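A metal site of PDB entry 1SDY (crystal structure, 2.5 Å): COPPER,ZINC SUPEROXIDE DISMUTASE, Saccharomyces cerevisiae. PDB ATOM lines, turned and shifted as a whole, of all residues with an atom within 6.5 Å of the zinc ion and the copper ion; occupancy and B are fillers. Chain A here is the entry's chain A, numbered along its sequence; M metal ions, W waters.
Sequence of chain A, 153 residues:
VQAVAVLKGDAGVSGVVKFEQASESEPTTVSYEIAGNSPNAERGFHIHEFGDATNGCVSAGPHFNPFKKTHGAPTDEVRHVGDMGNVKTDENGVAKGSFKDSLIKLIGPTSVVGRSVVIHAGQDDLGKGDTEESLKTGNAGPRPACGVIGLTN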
ATOM      1  N   GLY A  44      14.566  27.805 -21.149  1.00  0.00           N
ATOM      2  CA  GLY A  44      15.565  27.546 -22.189  1.00  0.00           C
ATOM      3  C   GLY A  44      15.853  28.713 -23.103  1.00  0.00           C
ATOM      4  O   GLY A  44      14.938  29.403 -23.509  1.00  0.00           O
ATOM      5  N   PHE A  45      17.131  28.936 -23.440  1.00  0.00           N
ATOM      6  CA  PHE A  45      17.500  30.116 -24.205  1.00  0.00           C
ATOM      7  C   PHE A  45      18.529  29.693 -25.201  1.00  0.00           C
ATOM      8  O   PHE A  45      19.661  29.408 -24.836  1.00  0.00           O
ATOM      9  CB  PHE A  45      18.067  31.128 -23.184  1.00  0.00           C
ATOM     10  CG  PHE A  45      18.484  32.469 -23.683  1.00  0.00           C
ATOM     11  CD1 PHE A  45      17.550  33.270 -24.349  1.00  0.00           C
ATOM     12  CD2 PHE A  45      19.743  32.972 -23.357  1.00  0.00           C
ATOM     13  CE1 PHE A  45      17.862  34.584 -24.702  1.00  0.00           C
ATOM     14  CE2 PHE A  45      20.066  34.291 -23.683  1.00  0.00           C
ATOM     15  CZ  PHE A  45      19.115  35.084 -24.325  1.00  0.00           C
ATOM     16  N   HIS A  46      18.105  29.784 -26.449  1.00  0.00           N
ATOM     17  CA  HIS A  46      18.886  29.323 -27.567  1.00  0.00           C
ATOM     18  C   HIS A  46      18.860  30.178 -28.813  1.00  0.00           C
ATOM     19  O   HIS A  46      17.982  30.975 -29.061  1.00  0.00           O
ATOM     20  CB  HIS A  46      18.186  28.028 -28.044  1.00  0.00           C
ATOM     21  CG  HIS A  46      17.807  27.085 -26.954  1.00  0.00           C
ATOM     22  ND1 HIS A  46      16.628  26.345 -27.019  1.00  0.00           N
ATOM     23  CD2 HIS A  46      18.468  26.712 -25.829  1.00  0.00           C
ATOM     24  CE1 HIS A  46      16.587  25.564 -25.948  1.00  0.00           C
ATOM     25  NE2 HIS A  46      17.698  25.733 -25.221  1.00  0.00           N
ATOM     26  N   ILE A  47      19.793  29.860 -29.664  1.00  0.00           N
ATOM     27  CA  ILE A  47      19.916  30.382 -30.964  1.00  0.00           C
ATOM     28  C   ILE A  47      19.547  29.251 -31.915  1.00  0.00           C
ATOM     29  O   ILE A  47      20.117  28.150 -31.914  1.00  0.00           O
ATOM     30  CB  ILE A  47      21.304  30.933 -31.307  1.00  0.00           C
ATOM     31  CG1 ILE A  47      21.509  32.285 -30.574  1.00  0.00           C
ATOM     32  CG2 ILE A  47      21.270  31.115 -32.826  1.00  0.00           C
ATOM     33  CD1 ILE A  47      22.936  32.695 -30.229  1.00  0.00           C
ATOM     34  N   HIS A  48      18.498  29.506 -32.674  1.00  0.00           N
ATOM     35  CA  HIS A  48      17.912  28.637 -33.664  1.00  0.00           C
ATOM     36  C   HIS A  48      18.471  29.141 -35.007  1.00  0.00           C
ATOM     37  O   HIS A  48      18.884  30.303 -35.167  1.00  0.00           O
ATOM     38  CB  HIS A  48      16.333  28.690 -33.612  1.00  0.00           C
ATOM     39  CG  HIS A  48      15.763  27.949 -32.486  1.00  0.00           C
ATOM     40  ND1 HIS A  48      14.976  26.820 -32.718  1.00  0.00           N
ATOM     41  CD2 HIS A  48      15.911  28.116 -31.139  1.00  0.00           C
ATOM     42  CE1 HIS A  48      14.680  26.319 -31.507  1.00  0.00           C
ATOM     43  NE2 HIS A  48      15.220  27.077 -30.545  1.00  0.00           N
ATOM     44  N   GLY A  61      13.289  27.346 -37.058  1.00  0.00           N
ATOM     45  CA  GLY A  61      13.898  26.071 -37.156  1.00  0.00           C
ATOM     46  C   GLY A  61      14.490  25.524 -35.844  1.00  0.00           C
ATOM     47  O   GLY A  61      14.151  25.901 -34.705  1.00  0.00           O
ATOM     48  N   PRO A  62      15.449  24.621 -36.040  1.00  0.00           N
ATOM     49  CA  PRO A  62      16.056  23.936 -34.936  1.00  0.00           C
ATOM     50  C   PRO A  62      17.200  24.762 -34.400  1.00  0.00           C
ATOM     51  O   PRO A  62      17.356  25.898 -34.774  1.00  0.00           O
ATOM     52  CB  PRO A  62      16.559  22.620 -35.528  1.00  0.00           C
ATOM     53  CG  PRO A  62      16.822  22.925 -37.023  1.00  0.00           C
ATOM     54  CD  PRO A  62      15.990  24.144 -37.382  1.00  0.00           C
ATOM     55  N   HIS A  63      17.987  24.199 -33.470  1.00  0.00           N
ATOM     56  CA  HIS A  63      19.086  24.942 -32.901  1.00  0.00           C
ATOM     57  C   HIS A  63      20.237  25.117 -33.866  1.00  0.00           C
ATOM     58  O   HIS A  63      20.582  24.169 -34.556  1.00  0.00           O
ATOM     59  CB  HIS A  63      19.597  24.140 -31.715  1.00  0.00           C
ATOM     60  CG  HIS A  63      18.692  24.189 -30.540  1.00  0.00           C
ATOM     61  ND1 HIS A  63      19.003  23.465 -29.405  1.00  0.00           N
ATOM     62  CD2 HIS A  63      17.534  24.871 -30.352  1.00  0.00           C
ATOM     63  CE1 HIS A  63      18.037  23.735 -28.547  1.00  0.00           C
ATOM     64  NE2 HIS A  63      17.140  24.576 -29.070  1.00  0.00           N
ATOM     65  N   PHE A  64      20.808  26.322 -33.999  1.00  0.00           N
ATOM     66  CA  PHE A  64      21.916  26.464 -34.929  1.00  0.00           C
ATOM     67  C   PHE A  64      22.986  25.484 -34.426  1.00  0.00           C
ATOM     68  O   PHE A  64      23.325  25.509 -33.248  1.00  0.00           O
ATOM     69  CB  PHE A  64      22.462  27.847 -34.793  1.00  0.00           C
ATOM     70  CG  PHE A  64      23.651  28.162 -35.639  1.00  0.00           C
ATOM     71  CD1 PHE A  64      23.634  27.863 -37.004  1.00  0.00           C
ATOM     72  CD2 PHE A  64      24.772  28.803 -35.118  1.00  0.00           C
ATOM     73  CE1 PHE A  64      24.669  28.261 -37.842  1.00  0.00           C
ATOM     74  CE2 PHE A  64      25.870  29.142 -35.926  1.00  0.00           C
ATOM     75  CZ  PHE A  64      25.795  28.884 -37.298  1.00  0.00           C
ATOM     76  N   THR A  70      25.256  17.125 -30.574  1.00  0.00           N
ATOM     77  CA  THR A  70      23.983  16.990 -29.903  1.00  0.00           C
ATOM     78  C   THR A  70      23.831  18.161 -28.914  1.00  0.00           C
ATOM     79  O   THR A  70      24.798  18.883 -28.504  1.00  0.00           O
ATOM     80  CB  THR A  70      23.844  15.623 -29.157  1.00  0.00           C
ATOM     81  OG1 THR A  70      25.009  15.336 -28.410  1.00  0.00           O
ATOM     82  CG2 THR A  70      23.629  14.433 -30.084  1.00  0.00           C
ATOM     83  N   HIS A  71      22.607  18.310 -28.454  1.00  0.00           N
ATOM     84  CA  HIS A  71      22.262  19.340 -27.487  1.00  0.00           C
ATOM     85  C   HIS A  71      22.978  19.133 -26.133  1.00  0.00           C
ATOM     86  O   HIS A  71      23.211  18.026 -25.674  1.00  0.00           O
ATOM     87  CB  HIS A  71      20.706  19.409 -27.388  1.00  0.00           C
ATOM     88  CG  HIS A  71      20.245  20.501 -26.476  1.00  0.00           C
ATOM     89  ND1 HIS A  71      20.142  21.827 -26.903  1.00  0.00           N
ATOM     90  CD2 HIS A  71      19.916  20.458 -25.146  1.00  0.00           C
ATOM     91  CE1 HIS A  71      19.754  22.534 -25.851  1.00  0.00           C
ATOM     92  NE2 HIS A  71      19.603  21.742 -24.777  1.00  0.00           N
ATOM     93  N   GLY A  72      23.372  20.208 -25.471  1.00  0.00           N
ATOM     94  CA  GLY A  72      24.089  20.129 -24.222  1.00  0.00           C
ATOM     95  C   GLY A  72      23.957  21.480 -23.509  1.00  0.00           C
ATOM     96  O   GLY A  72      23.186  22.345 -23.922  1.00  0.00           O
ATOM     97  N   ARG A  79      27.833  20.155 -27.601  1.00  0.00           N
ATOM     98  CA  ARG A  79      26.679  21.016 -27.516  1.00  0.00           C
ATOM     99  C   ARG A  79      26.504  21.682 -28.832  1.00  0.00           C
ATOM    100  O   ARG A  79      27.505  21.791 -29.532  1.00  0.00           O
ATOM    101  CB  ARG A  79      26.970  22.146 -26.525  1.00  0.00           C
ATOM    102  CG  ARG A  79      28.185  23.020 -26.867  1.00  0.00           C
ATOM    103  CD  ARG A  79      28.111  24.350 -26.106  1.00  0.00           C
ATOM    104  NE  ARG A  79      27.497  25.471 -26.840  1.00  0.00           N
ATOM    105  CZ  ARG A  79      27.802  26.736 -26.525  1.00  0.00           C
ATOM    106  NH1 ARG A  79      28.617  26.988 -25.538  1.00  0.00           N
ATOM    107  NH2 ARG A  79      27.354  27.795 -27.214  1.00  0.00           N
ATOM    108  N   HIS A  80      25.302  22.209 -29.089  1.00  0.00           N
ATOM    109  CA  HIS A  80      25.083  23.038 -30.262  1.00  0.00           C
ATOM    110  C   HIS A  80      25.695  24.450 -30.011  1.00  0.00           C
ATOM    111  O   HIS A  80      25.821  24.904 -28.869  1.00  0.00           O
ATOM    112  CB  HIS A  80      23.605  23.215 -30.471  1.00  0.00           C
ATOM    113  CG  HIS A  80      22.858  21.940 -30.633  1.00  0.00           C
ATOM    114  ND1 HIS A  80      21.557  21.811 -30.160  1.00  0.00           N
ATOM    115  CD2 HIS A  80      23.230  20.794 -31.255  1.00  0.00           C
ATOM    116  CE1 HIS A  80      21.147  20.611 -30.517  1.00  0.00           C
ATOM    117  NE2 HIS A  80      22.119  20.004 -31.206  1.00  0.00           N
ATOM    118  N   GLY A  82      24.162  26.942 -30.764  1.00  0.00           N
ATOM    119  CA  GLY A  82      23.093  27.756 -30.239  1.00  0.00           C
ATOM    120  C   GLY A  82      22.706  27.588 -28.750  1.00  0.00           C
ATOM    121  O   GLY A  82      21.914  28.381 -28.234  1.00  0.00           O
ATOM    122  N   ASP A  83      23.162  26.528 -28.090  1.00  0.00           N
ATOM    123  CA  ASP A  83      22.787  26.157 -26.730  1.00  0.00           C
ATOM    124  C   ASP A  83      23.250  27.198 -25.677  1.00  0.00           C
ATOM    125  O   ASP A  83      24.423  27.230 -25.312  1.00  0.00           O
ATOM    126  CB  ASP A  83      23.305  24.700 -26.433  1.00  0.00           C
ATOM    127  CG  ASP A  83      22.592  23.679 -27.285  1.00  0.00           C
ATOM    128  OD1 ASP A  83      21.491  23.988 -27.833  1.00  0.00           O
ATOM    129  OD2 ASP A  83      23.092  22.537 -27.461  1.00  0.00           O
ATOM    130  N   VAL A 118      15.690  32.419 -29.450  1.00  0.00           N
ATOM    131  CA  VAL A 118      14.529  31.799 -28.845  1.00  0.00           C
ATOM    132  C   VAL A 118      14.472  31.747 -27.318  1.00  0.00           C
ATOM    133  O   VAL A 118      15.449  31.303 -26.685  1.00  0.00           O
ATOM    134  CB  VAL A 118      13.493  31.068 -29.719  1.00  0.00           C
ATOM    135  CG1 VAL A 118      14.041  30.397 -30.985  1.00  0.00           C
ATOM    136  CG2 VAL A 118      12.703  30.067 -28.916  1.00  0.00           C
ATOM    137  N   HIS A 120      12.210  30.025 -24.475  1.00  0.00           N
ATOM    138  CA  HIS A 120      11.226  28.964 -24.386  1.00  0.00           C
ATOM    139  C   HIS A 120      10.259  29.098 -23.194  1.00  0.00           C
ATOM    140  O   HIS A 120      10.513  29.810 -22.222  1.00  0.00           O
ATOM    141  CB  HIS A 120      11.967  27.625 -24.238  1.00  0.00           C
ATOM    142  CG  HIS A 120      12.540  27.236 -25.527  1.00  0.00           C
ATOM    143  ND1 HIS A 120      11.758  26.606 -26.464  1.00  0.00           N
ATOM    144  CD2 HIS A 120      13.814  27.347 -25.995  1.00  0.00           C
ATOM    145  CE1 HIS A 120      12.535  26.394 -27.521  1.00  0.00           C
ATOM    146  NE2 HIS A 120      13.773  26.851 -27.282  1.00  0.00           N
ATOM    147  N   ASP A 124      15.355  23.997 -19.978  1.00  0.00           N
ATOM    148  CA  ASP A 124      16.149  23.162 -20.803  1.00  0.00           C
ATOM    149  C   ASP A 124      16.788  22.079 -19.939  1.00  0.00           C
ATOM    150  O   ASP A 124      17.573  22.403 -19.056  1.00  0.00           O
ATOM    151  CB  ASP A 124      17.220  24.059 -21.358  1.00  0.00           C
ATOM    152  CG  ASP A 124      18.097  23.363 -22.388  1.00  0.00           C
ATOM    153  OD1 ASP A 124      18.236  22.108 -22.356  1.00  0.00           O
ATOM    154  OD2 ASP A 124      18.757  24.124 -23.136  1.00  0.00           O
ATOM    155  N   SER A 134      15.709  15.138 -25.703  1.00  0.00           N
ATOM    156  CA  SER A 134      16.601  15.857 -24.861  1.00  0.00           C
ATOM    157  C   SER A 134      17.897  16.208 -25.583  1.00  0.00           C
ATOM    158  O   SER A 134      18.495  17.301 -25.485  1.00  0.00           O
ATOM    159  CB  SER A 134      16.976  15.027 -23.656  1.00  0.00           C
ATOM    160  OG  SER A 134      18.270  15.479 -23.248  1.00  0.00           O
ATOM    161  N   LEU A 135      18.299  15.201 -26.321  1.00  0.00           N
ATOM    162  CA  LEU A 135      19.468  15.269 -27.141  1.00  0.00           C
ATOM    163  C   LEU A 135      19.306  16.235 -28.346  1.00  0.00           C
ATOM    164  O   LEU A 135      20.295  16.642 -28.996  1.00  0.00           O
ATOM    165  CB  LEU A 135      19.841  13.840 -27.564  1.00  0.00           C
ATOM    166  CG  LEU A 135      21.010  13.291 -26.769  1.00  0.00           C
ATOM    167  CD1 LEU A 135      21.068  14.072 -25.463  1.00  0.00           C
ATOM    168  CD2 LEU A 135      20.860  11.792 -26.522  1.00  0.00           C
ATOM    169  N   LYS A 136      18.063  16.615 -28.649  1.00  0.00           N
ATOM    170  CA  LYS A 136      17.734  17.517 -29.779  1.00  0.00           C
ATOM    171  C   LYS A 136      17.457  18.974 -29.380  1.00  0.00           C
ATOM    172  O   LYS A 136      18.062  19.948 -29.905  1.00  0.00           O
ATOM    173  CB  LYS A 136      16.470  17.006 -30.425  1.00  0.00           C
ATOM    174  CG  LYS A 136      16.698  15.907 -31.462  1.00  0.00           C
ATOM    175  N   THR A 137      16.560  19.074 -28.389  1.00  0.00           N
ATOM    176  CA  THR A 137      16.090  20.347 -27.851  1.00  0.00           C
ATOM    177  C   THR A 137      16.191  20.579 -26.336  1.00  0.00           C
ATOM    178  O   THR A 137      15.790  21.651 -25.833  1.00  0.00           O
ATOM    179  CB  THR A 137      14.607  20.463 -28.239  1.00  0.00           C
ATOM    180  OG1 THR A 137      13.800  19.524 -27.512  1.00  0.00           O
ATOM    181  CG2 THR A 137      14.552  20.149 -29.714  1.00  0.00           C
ATOM    182  N   GLY A 138      16.667  19.573 -25.583  1.00  0.00           N
ATOM    183  CA  GLY A 138      16.704  19.733 -24.113  1.00  0.00           C
ATOM    184  C   GLY A 138      15.300  19.814 -23.512  1.00  0.00           C
ATOM    185  O   GLY A 138      15.119  20.179 -22.326  1.00  0.00           O
ATOM    186  N   ALA A 140      12.913  21.839 -24.060  1.00  0.00           N
ATOM    187  CA  ALA A 140      12.586  23.145 -23.578  1.00  0.00           C
ATOM    188  C   ALA A 140      11.151  23.565 -23.793  1.00  0.00           C
ATOM    189  O   ALA A 140      10.713  24.601 -23.312  1.00  0.00           O
ATOM    190  CB  ALA A 140      13.567  24.172 -24.126  1.00  0.00           C
ATOM    191  N   GLY A 141      10.395  22.844 -24.588  1.00  0.00           N
ATOM    192  CA  GLY A 141       9.036  23.326 -24.743  1.00  0.00           C
ATOM    193  C   GLY A 141       8.854  24.340 -25.852  1.00  0.00           C
ATOM    194  O   GLY A 141       9.757  24.569 -26.642  1.00  0.00           O
ATOM    195  N   ARG A 143       7.778  27.941 -27.916  1.00  0.00           N
ATOM    196  CA  ARG A 143       8.549  29.181 -28.022  1.00  0.00           C
ATOM    197  C   ARG A 143       7.688  30.426 -27.961  1.00  0.00           C
ATOM    198  O   ARG A 143       7.206  30.881 -28.979  1.00  0.00           O
ATOM    199  CB  ARG A 143       9.178  29.161 -29.403  1.00  0.00           C
ATOM    200  CG  ARG A 143       9.614  27.761 -29.854  1.00  0.00           C
ATOM    201  CD  ARG A 143       9.983  27.652 -31.342  1.00  0.00           C
ATOM    202  NE  ARG A 143      10.690  26.421 -31.765  1.00  0.00           N
ATOM    203  CZ  ARG A 143      11.361  26.248 -32.926  1.00  0.00           C
ATOM    204  NH1 ARG A 143      11.520  27.164 -33.913  1.00  0.00           N
ATOM    205  NH2 ARG A 143      11.942  25.066 -33.060  1.00  0.00           N
HETATM  206 ZN    ZN M   1      20.539  22.597 -28.596  1.00  0.00          ZN
HETATM  207 CU    CU M   2      15.555  26.349 -28.528  1.00  0.00          CU
HETATM  208  O   HOH W   1      14.554  24.856 -28.971  1.00  0.00           O
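The copper ion is bound by a ring nitrogen (ND1) of His 46, at 1.9 Å.
Water W1 binds the copper ion, at 1.9 Å.
The copper ion is bound by NE2 of His 48 (2.2 Å).
NE2 of His 120 is bound to the copper ion.
A ring nitrogen (NE2) of His 63 is bound to the copper ion (2.4 Å).
The zinc ion is bound by OD1 of Asp 83 (1.9 Å).
A ring nitrogen (ND1) of His 71 binds the zinc ion (1.9 Å).
The zinc ion is bound by a ring nitrogen (ND1) of His 63.
The zinc ion is bound by ND1 of His 80 (2.0 Å).
The zinc ion has four donor atoms within binding distance.
Slightly farther from the zinc ion lies OD2 of Asp 83 (2.8 Å).
N of Gly 72 lies within hydrogen-bond range of OD2 of Asp 83, at 3.1 Å.
O of His 46 sits at hydrogen-bond distance from N of Val 118.
A ring nitrogen (NE2) of His 46 sits at hydrogen-bond distance from the side-chain carboxylate of Asp 124 (2.8 Å).
N of His 71 is in hydrogen-bond range of O of Leu 135.
ND1 of His 48 sits close to O of Pro 62.
O of Thr 70 sits at hydrogen-bond distance from N of His 80 (3.4 Å).
The backbone carbonyl oxygen of Gly 44 sits at hydrogen-bond distance from the backbone NH of His 120, at 3.0 Å.
The backbone carbonyl oxygen (O) of Gly 141 lies within hydrogen-bond range of a ring nitrogen (ND1) of His 120 (2.9 Å).
Within 4 Å of the copper ion: His 46, His 48, His 63 and His 120.
The nearest printed residue that does not touch the copper ion is Val 118 (4.7 Å).
Merely in contact with the zinc ion: Lys 136 (3.9 Å).
Five residues have an atom within 4 Å of the zinc ion: His 63, His 71, His 80, Asp 83 and Lys 136.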
